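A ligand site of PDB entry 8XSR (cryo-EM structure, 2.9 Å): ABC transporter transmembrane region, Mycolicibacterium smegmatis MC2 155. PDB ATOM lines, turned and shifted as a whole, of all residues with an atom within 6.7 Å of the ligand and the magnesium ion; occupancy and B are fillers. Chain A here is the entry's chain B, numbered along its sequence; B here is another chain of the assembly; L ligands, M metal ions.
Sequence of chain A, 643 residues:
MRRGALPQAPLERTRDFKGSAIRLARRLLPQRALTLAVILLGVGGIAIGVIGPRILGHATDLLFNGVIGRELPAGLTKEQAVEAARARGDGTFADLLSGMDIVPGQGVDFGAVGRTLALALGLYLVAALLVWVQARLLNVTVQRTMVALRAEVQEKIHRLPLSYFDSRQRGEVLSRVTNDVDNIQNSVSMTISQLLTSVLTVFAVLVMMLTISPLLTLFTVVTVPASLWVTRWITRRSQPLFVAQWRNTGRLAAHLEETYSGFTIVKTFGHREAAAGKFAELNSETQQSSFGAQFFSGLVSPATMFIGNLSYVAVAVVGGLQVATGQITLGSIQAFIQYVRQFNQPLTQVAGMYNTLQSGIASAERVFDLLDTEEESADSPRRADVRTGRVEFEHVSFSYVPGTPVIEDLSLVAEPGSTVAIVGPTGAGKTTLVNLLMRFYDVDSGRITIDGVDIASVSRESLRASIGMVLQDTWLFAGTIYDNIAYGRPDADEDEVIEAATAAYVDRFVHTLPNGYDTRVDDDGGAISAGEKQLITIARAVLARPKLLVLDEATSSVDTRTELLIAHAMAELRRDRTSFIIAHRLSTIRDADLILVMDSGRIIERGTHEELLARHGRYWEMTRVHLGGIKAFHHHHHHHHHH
Residues that only touch the ligand: Tyr 400 (3.5 Å), Val 406 (3.6 Å), Thr 426 (3.7 Å), Pro 425 (3.7 Å), Tyr 441 (3.8 Å) and Ala 428 (3.98 Å).
Hydrophobic or aromatic side chains that line the ligand: Tyr 400 and Val 406.
12 residues have an atom within 4 Å of the ligand: Asp 166, Tyr 400, Val 406, Pro 425, Thr 426, Gly 427, Ala 428, Gly 429, Lys 430, Thr 431, Thr 432 and Tyr 441.
The nearest printed residue that does not touch the ligand is Leu 433 (5.1 Å).
An oxygen (O5) of the ligand sits at hydrogen-bond distance from the side-chain hydroxyl (OG1) of Thr 432, at 2.5 Å.
OD2 of Asp 166 lies within hydrogen-bond range of N3 of the ligand, at 3.3 Å.
The backbone NH (N) of Thr 432 lies within hydrogen-bond range of an oxygen (O5) of the ligand.
N of Gly 427 lies within hydrogen-bond range of O3 of the ligand (2.8 Å).
O6 of the ligand lies within hydrogen-bond range of N of Gly 429, 3.2 Å away.
An oxygen (O1) of the ligand sits close to the backbone NH (N) of Thr 431.
The backbone NH (N) of Lys 430 sits at hydrogen-bond distance from an oxygen (O6) of the ligand (3.1 Å).
The magnesium ion is bound by OG1 of Thr 431 (2.1 Å) and O1 of the ligand (2.1 Å).
The magnesium ion has two donor atoms within binding distance.
The side-chain hydroxyl (OH) of Tyr 441 lies close to the side-chain carboxylate (OD1) of Asp 166 (3.1 Å).
OH of Tyr 400 is in hydrogen-bond range of OG1 of Thr 432, at 2.5 Å.
OE1 of Glu 553 lies close to OE1 of Gln 472 (2.7 Å).
The backbone carbonyl oxygen of Leu 162 sits close to the side-chain carboxylate of Asp 166.
The side-chain hydroxyl of Thr 431 lies close to the side-chain carboxylate of Asp 552 (3.2 Å).
O of Ile 582 lies within hydrogen-bond range of N of Glu 553 (2.8 Å).
The backbone carbonyl oxygen (O) of Asp 552 lies within hydrogen-bond range of the backbone NH (N) of Gln 472 (2.9 Å).
OD2 of Asp 166 is in salt-bridge range of NH1 of Arg 211 of chain B, at 3.4 Å.
Residues that only touch the magnesium ion: Asp 552 and Glu 553.
Within 4 Å of the magnesium ion: Thr 431, Asp 552 and Glu 553.
The nearest printed residue that does not touch the magnesium ion is Gln 472 (4.02 Å).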
ATOM      1  N   LEU A 162     -18.047 -11.233  -0.598  1.00  0.00           N
ATOM      2  CA  LEU A 162     -17.214 -12.073  -1.442  1.00  0.00           C
ATOM      3  C   LEU A 162     -15.752 -11.665  -1.437  1.00  0.00           C
ATOM      4  O   LEU A 162     -14.895 -12.485  -1.755  1.00  0.00           O
ATOM      5  CB  LEU A 162     -17.723 -12.068  -2.886  1.00  0.00           C
ATOM      6  CG  LEU A 162     -18.808 -13.085  -3.266  1.00  0.00           C
ATOM      7  CD1 LEU A 162     -18.348 -14.498  -2.968  1.00  0.00           C
ATOM      8  CD2 LEU A 162     -20.126 -12.783  -2.605  1.00  0.00           C
ATOM      9  N   SER A 163     -15.448 -10.416  -1.073  1.00  0.00           N
ATOM     10  CA  SER A 163     -14.070  -9.951  -0.991  1.00  0.00           C
ATOM     11  C   SER A 163     -13.302 -10.619   0.145  1.00  0.00           C
ATOM     12  O   SER A 163     -12.078 -10.495   0.197  1.00  0.00           O
ATOM     13  CB  SER A 163     -14.040  -8.438  -0.822  1.00  0.00           C
ATOM     14  OG  SER A 163     -14.586  -8.056   0.429  1.00  0.00           O
ATOM     15  N   ASP A 166     -12.209 -14.657  -1.558  1.00  0.00           N
ATOM     16  CA  ASP A 166     -11.282 -14.744  -2.675  1.00  0.00           C
ATOM     17  C   ASP A 166     -10.055 -13.871  -2.474  1.00  0.00           C
ATOM     18  O   ASP A 166      -9.235 -13.749  -3.395  1.00  0.00           O
ATOM     19  CB  ASP A 166     -11.998 -14.393  -3.977  1.00  0.00           C
ATOM     20  CG  ASP A 166     -12.600 -13.003  -3.967  1.00  0.00           C
ATOM     21  OD1 ASP A 166     -12.461 -12.299  -2.951  1.00  0.00           O
ATOM     22  OD2 ASP A 166     -13.223 -12.625  -4.979  1.00  0.00           O
ATOM     23  N   SER A 167      -9.897 -13.268  -1.302  1.00  0.00           N
ATOM     24  CA  SER A 167      -8.656 -12.603  -0.915  1.00  0.00           C
ATOM     25  C   SER A 167      -7.840 -13.445   0.048  1.00  0.00           C
ATOM     26  O   SER A 167      -6.761 -13.024   0.459  1.00  0.00           O
ATOM     27  CB  SER A 167      -8.954 -11.237  -0.296  1.00  0.00           C
ATOM     28  OG  SER A 167      -9.612 -11.385   0.950  1.00  0.00           O
ATOM     29  N   TYR A 400     -10.833  -3.412  -7.537  1.00  0.00           N
ATOM     30  CA  TYR A 400     -10.715  -4.352  -6.435  1.00  0.00           C
ATOM     31  C   TYR A 400      -9.861  -3.782  -5.315  1.00  0.00           C
ATOM     32  O   TYR A 400     -10.350  -3.575  -4.186  1.00  0.00           O
ATOM     33  CB  TYR A 400     -10.135  -5.677  -6.911  1.00  0.00           C
ATOM     34  CG  TYR A 400     -11.064  -6.497  -7.779  1.00  0.00           C
ATOM     35  CD1 TYR A 400     -12.079  -7.243  -7.207  1.00  0.00           C
ATOM     36  CD2 TYR A 400     -10.905  -6.553  -9.150  1.00  0.00           C
ATOM     37  CE1 TYR A 400     -12.925  -7.999  -7.994  1.00  0.00           C
ATOM     38  CE2 TYR A 400     -11.743  -7.303  -9.937  1.00  0.00           C
ATOM     39  CZ  TYR A 400     -12.755  -8.025  -9.348  1.00  0.00           C
ATOM     40  OH  TYR A 400     -13.599  -8.784 -10.125  1.00  0.00           O
ATOM     41  N   VAL A 401      -8.588  -3.523  -5.591  1.00  0.00           N
ATOM     42  CA  VAL A 401      -7.685  -2.899  -4.634  1.00  0.00           C
ATOM     43  C   VAL A 401      -7.493  -1.458  -5.073  1.00  0.00           C
ATOM     44  O   VAL A 401      -7.326  -1.192  -6.266  1.00  0.00           O
ATOM     45  CB  VAL A 401      -6.357  -3.683  -4.535  1.00  0.00           C
ATOM     46  CG1 VAL A 401      -5.645  -3.726  -5.875  1.00  0.00           C
ATOM     47  CG2 VAL A 401      -5.457  -3.083  -3.478  1.00  0.00           C
ATOM     48  N   PRO A 405      -7.441   0.605 -11.370  1.00  0.00           N
ATOM     49  CA  PRO A 405      -8.763   0.477 -12.003  1.00  0.00           C
ATOM     50  C   PRO A 405      -8.908  -0.855 -12.723  1.00  0.00           C
ATOM     51  O   PRO A 405      -7.997  -1.346 -13.370  1.00  0.00           O
ATOM     52  CB  PRO A 405      -8.794   1.656 -12.990  1.00  0.00           C
ATOM     53  CG  PRO A 405      -7.808   2.630 -12.445  1.00  0.00           C
ATOM     54  CD  PRO A 405      -6.719   1.789 -11.851  1.00  0.00           C
ATOM     55  N   VAL A 406     -10.103  -1.434 -12.587  1.00  0.00           N
ATOM     56  CA  VAL A 406     -10.421  -2.696 -13.241  1.00  0.00           C
ATOM     57  C   VAL A 406     -11.550  -2.438 -14.243  1.00  0.00           C
ATOM     58  O   VAL A 406     -11.627  -3.088 -15.285  1.00  0.00           O
ATOM     59  CB  VAL A 406     -10.817  -3.769 -12.206  1.00  0.00           C
ATOM     60  CG1 VAL A 406     -11.276  -5.031 -12.888  1.00  0.00           C
ATOM     61  CG2 VAL A 406      -9.635  -4.062 -11.301  1.00  0.00           C
ATOM     62  N   GLY A 424     -13.764  -9.926 -25.613  1.00  0.00           N
ATOM     63  CA  GLY A 424     -12.535  -9.239 -25.292  1.00  0.00           C
ATOM     64  C   GLY A 424     -11.457 -10.179 -24.782  1.00  0.00           C
ATOM     65  O   GLY A 424     -11.681 -11.383 -24.623  1.00  0.00           O
ATOM     66  N   PRO A 425     -10.267  -9.640 -24.524  1.00  0.00           N
ATOM     67  CA  PRO A 425      -9.161 -10.472 -24.037  1.00  0.00           C
ATOM     68  C   PRO A 425      -9.390 -10.983 -22.636  1.00  0.00           C
ATOM     69  O   PRO A 425     -10.439 -10.726 -22.029  1.00  0.00           O
ATOM     70  CB  PRO A 425      -7.955  -9.530 -24.099  1.00  0.00           C
ATOM     71  CG  PRO A 425      -8.353  -8.465 -25.066  1.00  0.00           C
ATOM     72  CD  PRO A 425      -9.815  -8.282 -24.867  1.00  0.00           C
ATOM     73  N   THR A 426      -8.414 -11.717 -22.093  1.00  0.00           N
ATOM     74  CA  THR A 426      -8.465 -12.186 -20.710  1.00  0.00           C
ATOM     75  C   THR A 426      -7.836 -11.128 -19.827  1.00  0.00           C
ATOM     76  O   THR A 426      -6.697 -10.701 -20.077  1.00  0.00           O
ATOM     77  CB  THR A 426      -7.749 -13.527 -20.554  1.00  0.00           C
ATOM     78  OG1 THR A 426      -8.374 -14.503 -21.389  1.00  0.00           O
ATOM     79  CG2 THR A 426      -7.803 -13.984 -19.113  1.00  0.00           C
ATOM     80  N   GLY A 427      -8.561 -10.712 -18.800  1.00  0.00           N
ATOM     81  CA  GLY A 427      -8.163  -9.596 -17.963  1.00  0.00           C
ATOM     82  C   GLY A 427      -8.827  -8.291 -18.333  1.00  0.00           C
ATOM     83  O   GLY A 427      -8.565  -7.274 -17.664  1.00  0.00           O
ATOM     84  N   ALA A 428      -9.666  -8.274 -19.360  1.00  0.00           N
ATOM     85  CA  ALA A 428     -10.338  -7.050 -19.754  1.00  0.00           C
ATOM     86  C   ALA A 428     -11.338  -6.579 -18.702  1.00  0.00           C
ATOM     87  O   ALA A 428     -11.734  -5.412 -18.707  1.00  0.00           O
ATOM     88  CB  ALA A 428     -11.036  -7.237 -21.098  1.00  0.00           C
ATOM     89  N   GLY A 429     -11.764  -7.476 -17.818  1.00  0.00           N
ATOM     90  CA  GLY A 429     -12.741  -7.135 -16.812  1.00  0.00           C
ATOM     91  C   GLY A 429     -14.141  -7.586 -17.195  1.00  0.00           C
ATOM     92  O   GLY A 429     -15.126  -6.907 -16.889  1.00  0.00           O
ATOM     93  N   LYS A 430     -14.226  -8.731 -17.864  1.00  0.00           N
ATOM     94  CA  LYS A 430     -15.513  -9.280 -18.279  1.00  0.00           C
ATOM     95  C   LYS A 430     -16.229  -9.977 -17.137  1.00  0.00           C
ATOM     96  O   LYS A 430     -17.431  -9.774 -16.937  1.00  0.00           O
ATOM     97  CB  LYS A 430     -15.320 -10.261 -19.436  1.00  0.00           C
ATOM     98  CG  LYS A 430     -14.802  -9.625 -20.700  1.00  0.00           C
ATOM     99  CD  LYS A 430     -14.741 -10.642 -21.824  1.00  0.00           C
ATOM    100  CE  LYS A 430     -13.590 -11.604 -21.602  1.00  0.00           C
ATOM    101  NZ  LYS A 430     -13.428 -12.554 -22.732  1.00  0.00           N
ATOM    102  N   THR A 431     -15.518 -10.814 -16.377  1.00  0.00           N
ATOM    103  CA  THR A 431     -16.091 -11.451 -15.210  1.00  0.00           C
ATOM    104  C   THR A 431     -16.363 -10.466 -14.090  1.00  0.00           C
ATOM    105  O   THR A 431     -17.397 -10.571 -13.423  1.00  0.00           O
ATOM    106  CB  THR A 431     -15.162 -12.558 -14.696  1.00  0.00           C
ATOM    107  OG1 THR A 431     -14.982 -13.538 -15.733  1.00  0.00           O
ATOM    108  CG2 THR A 431     -15.753 -13.226 -13.471  1.00  0.00           C
ATOM    109  N   THR A 432     -15.459  -9.513 -13.858  1.00  0.00           N
ATOM    110  CA  THR A 432     -15.686  -8.454 -12.893  1.00  0.00           C
ATOM    111  C   THR A 432     -16.967  -7.690 -13.157  1.00  0.00           C
ATOM    112  O   THR A 432     -17.641  -7.295 -12.199  1.00  0.00           O
ATOM    113  CB  THR A 432     -14.499  -7.480 -12.909  1.00  0.00           C
ATOM    114  OG1 THR A 432     -13.325  -8.167 -12.504  1.00  0.00           O
ATOM    115  CG2 THR A 432     -14.744  -6.319 -11.982  1.00  0.00           C
ATOM    116  N   LEU A 433     -17.348  -7.503 -14.414  1.00  0.00           N
ATOM    117  CA  LEU A 433     -18.591  -6.850 -14.763  1.00  0.00           C
ATOM    118  C   LEU A 433     -19.805  -7.658 -14.315  1.00  0.00           C
ATOM    119  O   LEU A 433     -20.809  -7.062 -13.904  1.00  0.00           O
ATOM    120  CB  LEU A 433     -18.623  -6.623 -16.274  1.00  0.00           C
ATOM    121  CG  LEU A 433     -19.532  -5.534 -16.831  1.00  0.00           C
ATOM    122  CD1 LEU A 433     -19.019  -4.206 -16.329  1.00  0.00           C
ATOM    123  CD2 LEU A 433     -19.528  -5.565 -18.336  1.00  0.00           C
ATOM    124  N   ASN A 435     -19.618  -9.768 -11.622  1.00  0.00           N
ATOM    125  CA  ASN A 435     -19.565  -9.581 -10.182  1.00  0.00           C
ATOM    126  C   ASN A 435     -20.166  -8.257  -9.746  1.00  0.00           C
ATOM    127  O   ASN A 435     -20.550  -8.115  -8.583  1.00  0.00           O
ATOM    128  CB  ASN A 435     -18.122  -9.670  -9.674  1.00  0.00           C
ATOM    129  CG  ASN A 435     -17.566 -11.072  -9.775  1.00  0.00           C
ATOM    130  OD1 ASN A 435     -18.250 -12.046  -9.500  1.00  0.00           O
ATOM    131  ND2 ASN A 435     -16.301 -11.176 -10.148  1.00  0.00           N
ATOM    132  N   TYR A 441     -19.803  -7.368  -5.655  1.00  0.00           N
ATOM    133  CA  TYR A 441     -18.937  -6.266  -5.271  1.00  0.00           C
ATOM    134  C   TYR A 441     -19.687  -4.968  -5.521  1.00  0.00           C
ATOM    135  O   TYR A 441     -20.514  -4.887  -6.422  1.00  0.00           O
ATOM    136  CB  TYR A 441     -17.637  -6.269  -6.075  1.00  0.00           C
ATOM    137  CG  TYR A 441     -16.716  -7.422  -5.745  1.00  0.00           C
ATOM    138  CD1 TYR A 441     -15.849  -7.340  -4.660  1.00  0.00           C
ATOM    139  CD2 TYR A 441     -16.718  -8.578  -6.497  1.00  0.00           C
ATOM    140  CE1 TYR A 441     -15.008  -8.382  -4.353  1.00  0.00           C
ATOM    141  CE2 TYR A 441     -15.879  -9.633  -6.195  1.00  0.00           C
ATOM    142  CZ  TYR A 441     -15.033  -9.525  -5.118  1.00  0.00           C
ATOM    143  OH  TYR A 441     -14.193 -10.566  -4.812  1.00  0.00           O
ATOM    144  N   GLN A 472     -17.697 -19.452 -15.731  1.00  0.00           N
ATOM    145  CA  GLN A 472     -16.829 -20.359 -16.464  1.00  0.00           C
ATOM    146  C   GLN A 472     -16.426 -21.569 -15.631  1.00  0.00           C
ATOM    147  O   GLN A 472     -16.341 -22.680 -16.170  1.00  0.00           O
ATOM    148  CB  GLN A 472     -15.589 -19.622 -16.951  1.00  0.00           C
ATOM    149  CG  GLN A 472     -14.693 -20.452 -17.846  1.00  0.00           C
ATOM    150  CD  GLN A 472     -13.514 -19.671 -18.361  1.00  0.00           C
ATOM    151  OE1 GLN A 472     -13.320 -18.510 -17.995  1.00  0.00           O
ATOM    152  NE2 GLN A 472     -12.718 -20.297 -19.213  1.00  0.00           N
ATOM    153  N   ASP A 552     -21.406 -16.352 -18.470  1.00  0.00           N
ATOM    154  CA  ASP A 552     -20.024 -15.890 -18.401  1.00  0.00           C
ATOM    155  C   ASP A 552     -19.086 -17.049 -18.727  1.00  0.00           C
ATOM    156  O   ASP A 552     -18.504 -17.688 -17.847  1.00  0.00           O
ATOM    157  CB  ASP A 552     -19.721 -15.292 -17.043  1.00  0.00           C
ATOM    158  CG  ASP A 552     -18.301 -14.786 -16.934  1.00  0.00           C
ATOM    159  OD1 ASP A 552     -17.984 -13.747 -17.549  1.00  0.00           O
ATOM    160  OD2 ASP A 552     -17.495 -15.434 -16.236  1.00  0.00           O
ATOM    161  N   GLU A 553     -18.912 -17.300 -20.027  1.00  0.00           N
ATOM    162  CA  GLU A 553     -17.985 -18.302 -20.545  1.00  0.00           C
ATOM    163  C   GLU A 553     -18.216 -19.673 -19.916  1.00  0.00           C
ATOM    164  O   GLU A 553     -17.296 -20.468 -19.757  1.00  0.00           O
ATOM    165  CB  GLU A 553     -16.534 -17.857 -20.345  1.00  0.00           C
ATOM    166  CG  GLU A 553     -16.099 -16.710 -21.223  1.00  0.00           C
ATOM    167  CD  GLU A 553     -14.658 -16.305 -20.991  1.00  0.00           C
ATOM    168  OE1 GLU A 553     -14.028 -16.850 -20.067  1.00  0.00           O
ATOM    169  OE2 GLU A 553     -14.156 -15.448 -21.742  1.00  0.00           O
ATOM    170  N   ILE A 582     -20.899 -13.649 -22.366  1.00  0.00           N
ATOM    171  CA  ILE A 582     -19.478 -13.378 -22.366  1.00  0.00           C
ATOM    172  C   ILE A 582     -18.801 -14.624 -22.909  1.00  0.00           C
ATOM    173  O   ILE A 582     -18.817 -15.679 -22.258  1.00  0.00           O
ATOM    174  CB  ILE A 582     -18.973 -13.020 -20.964  1.00  0.00           C
ATOM    175  CG1 ILE A 582     -19.610 -11.701 -20.523  1.00  0.00           C
ATOM    176  CG2 ILE A 582     -17.463 -12.930 -20.954  1.00  0.00           C
ATOM    177  CD1 ILE A 582     -19.403 -11.385 -19.090  1.00  0.00           C
ATOM    178  N   ARG B 211     -20.534 -18.547  -4.076  1.00  0.00           N
ATOM    179  CA  ARG B 211     -20.948 -17.541  -5.038  1.00  0.00           C
ATOM    180  C   ARG B 211     -22.207 -17.945  -5.784  1.00  0.00           C
ATOM    181  O   ARG B 211     -23.048 -17.089  -6.066  1.00  0.00           O
ATOM    182  CB  ARG B 211     -19.804 -17.296  -6.021  1.00  0.00           C
ATOM    183  CG  ARG B 211     -19.941 -16.084  -6.892  1.00  0.00           C
ATOM    184  CD  ARG B 211     -18.735 -15.951  -7.795  1.00  0.00           C
ATOM    185  NE  ARG B 211     -17.494 -15.726  -7.040  1.00  0.00           N
ATOM    186  CZ  ARG B 211     -17.050 -14.531  -6.688  1.00  0.00           C
ATOM    187  NH1 ARG B 211     -15.920 -14.416  -6.002  1.00  0.00           N
ATOM    188  NH2 ARG B 211     -17.718 -13.439  -7.041  1.00  0.00           N
HETATM  189  P1  LIG L   1     -11.858 -11.742 -17.457  1.00  0.00           P
HETATM  190  O1  LIG L   1     -12.808 -12.739 -16.840  1.00  0.00           O
HETATM  191  O2  LIG L   1     -12.236 -11.268 -18.823  1.00  0.00           O
HETATM  192  O3  LIG L   1     -10.400 -12.114 -17.311  1.00  0.00           O
HETATM  193  P2  LIG L   1     -11.644 -10.368 -15.006  1.00  0.00           P
HETATM  194  O4  LIG L   1     -10.945 -11.640 -14.610  1.00  0.00           O
HETATM  195  O5  LIG L   1     -12.851  -9.915 -14.242  1.00  0.00           O
HETATM  196  O6  LIG L   1     -11.992 -10.412 -16.580  1.00  0.00           O
HETATM  197  O7  LIG L   1     -10.563  -9.183 -14.976  1.00  0.00           O
HETATM  198  C1  LIG L   1     -10.422  -8.373 -13.818  1.00  0.00           C
HETATM  199  C2  LIG L   1      -8.968  -8.009 -13.623  1.00  0.00           C
HETATM  200  O8  LIG L   1      -8.795  -7.724 -12.247  1.00  0.00           O
HETATM  201  C3  LIG L   1      -8.061  -9.178 -13.957  1.00  0.00           C
HETATM  202  O9  LIG L   1      -6.949  -8.721 -14.727  1.00  0.00           O
HETATM  203  C4  LIG L   1      -7.579  -9.736 -12.637  1.00  0.00           C
HETATM  204  O10 LIG L   1      -6.159  -9.845 -12.655  1.00  0.00           O
HETATM  205  C5  LIG L   1      -8.023  -8.726 -11.595  1.00  0.00           C
HETATM  206  N1  LIG L   1      -8.874  -9.405 -10.594  1.00  0.00           N
HETATM  207  C6  LIG L   1      -9.899 -10.226 -10.878  1.00  0.00           C
HETATM  208  N2  LIG L   1     -10.488 -10.687  -9.747  1.00  0.00           N
HETATM  209  C7  LIG L   1      -9.831 -10.155  -8.710  1.00  0.00           C
HETATM  210  C8  LIG L   1      -9.930 -10.227  -7.231  1.00  0.00           C
HETATM  211  N3  LIG L   1     -10.875 -10.980  -6.632  1.00  0.00           N
HETATM  212  N4  LIG L   1      -9.034  -9.521  -6.512  1.00  0.00           N
HETATM  213  C9  LIG L   1      -8.079  -8.764  -7.101  1.00  0.00           C
HETATM  214  N5  LIG L   1      -7.935  -8.655  -8.427  1.00  0.00           N
HETATM  215  C10 LIG L   1      -8.761  -9.320  -9.273  1.00  0.00           C
HETATM  216 MG    MG M   1     -13.627 -14.679 -16.813  1.00  0.00          MG
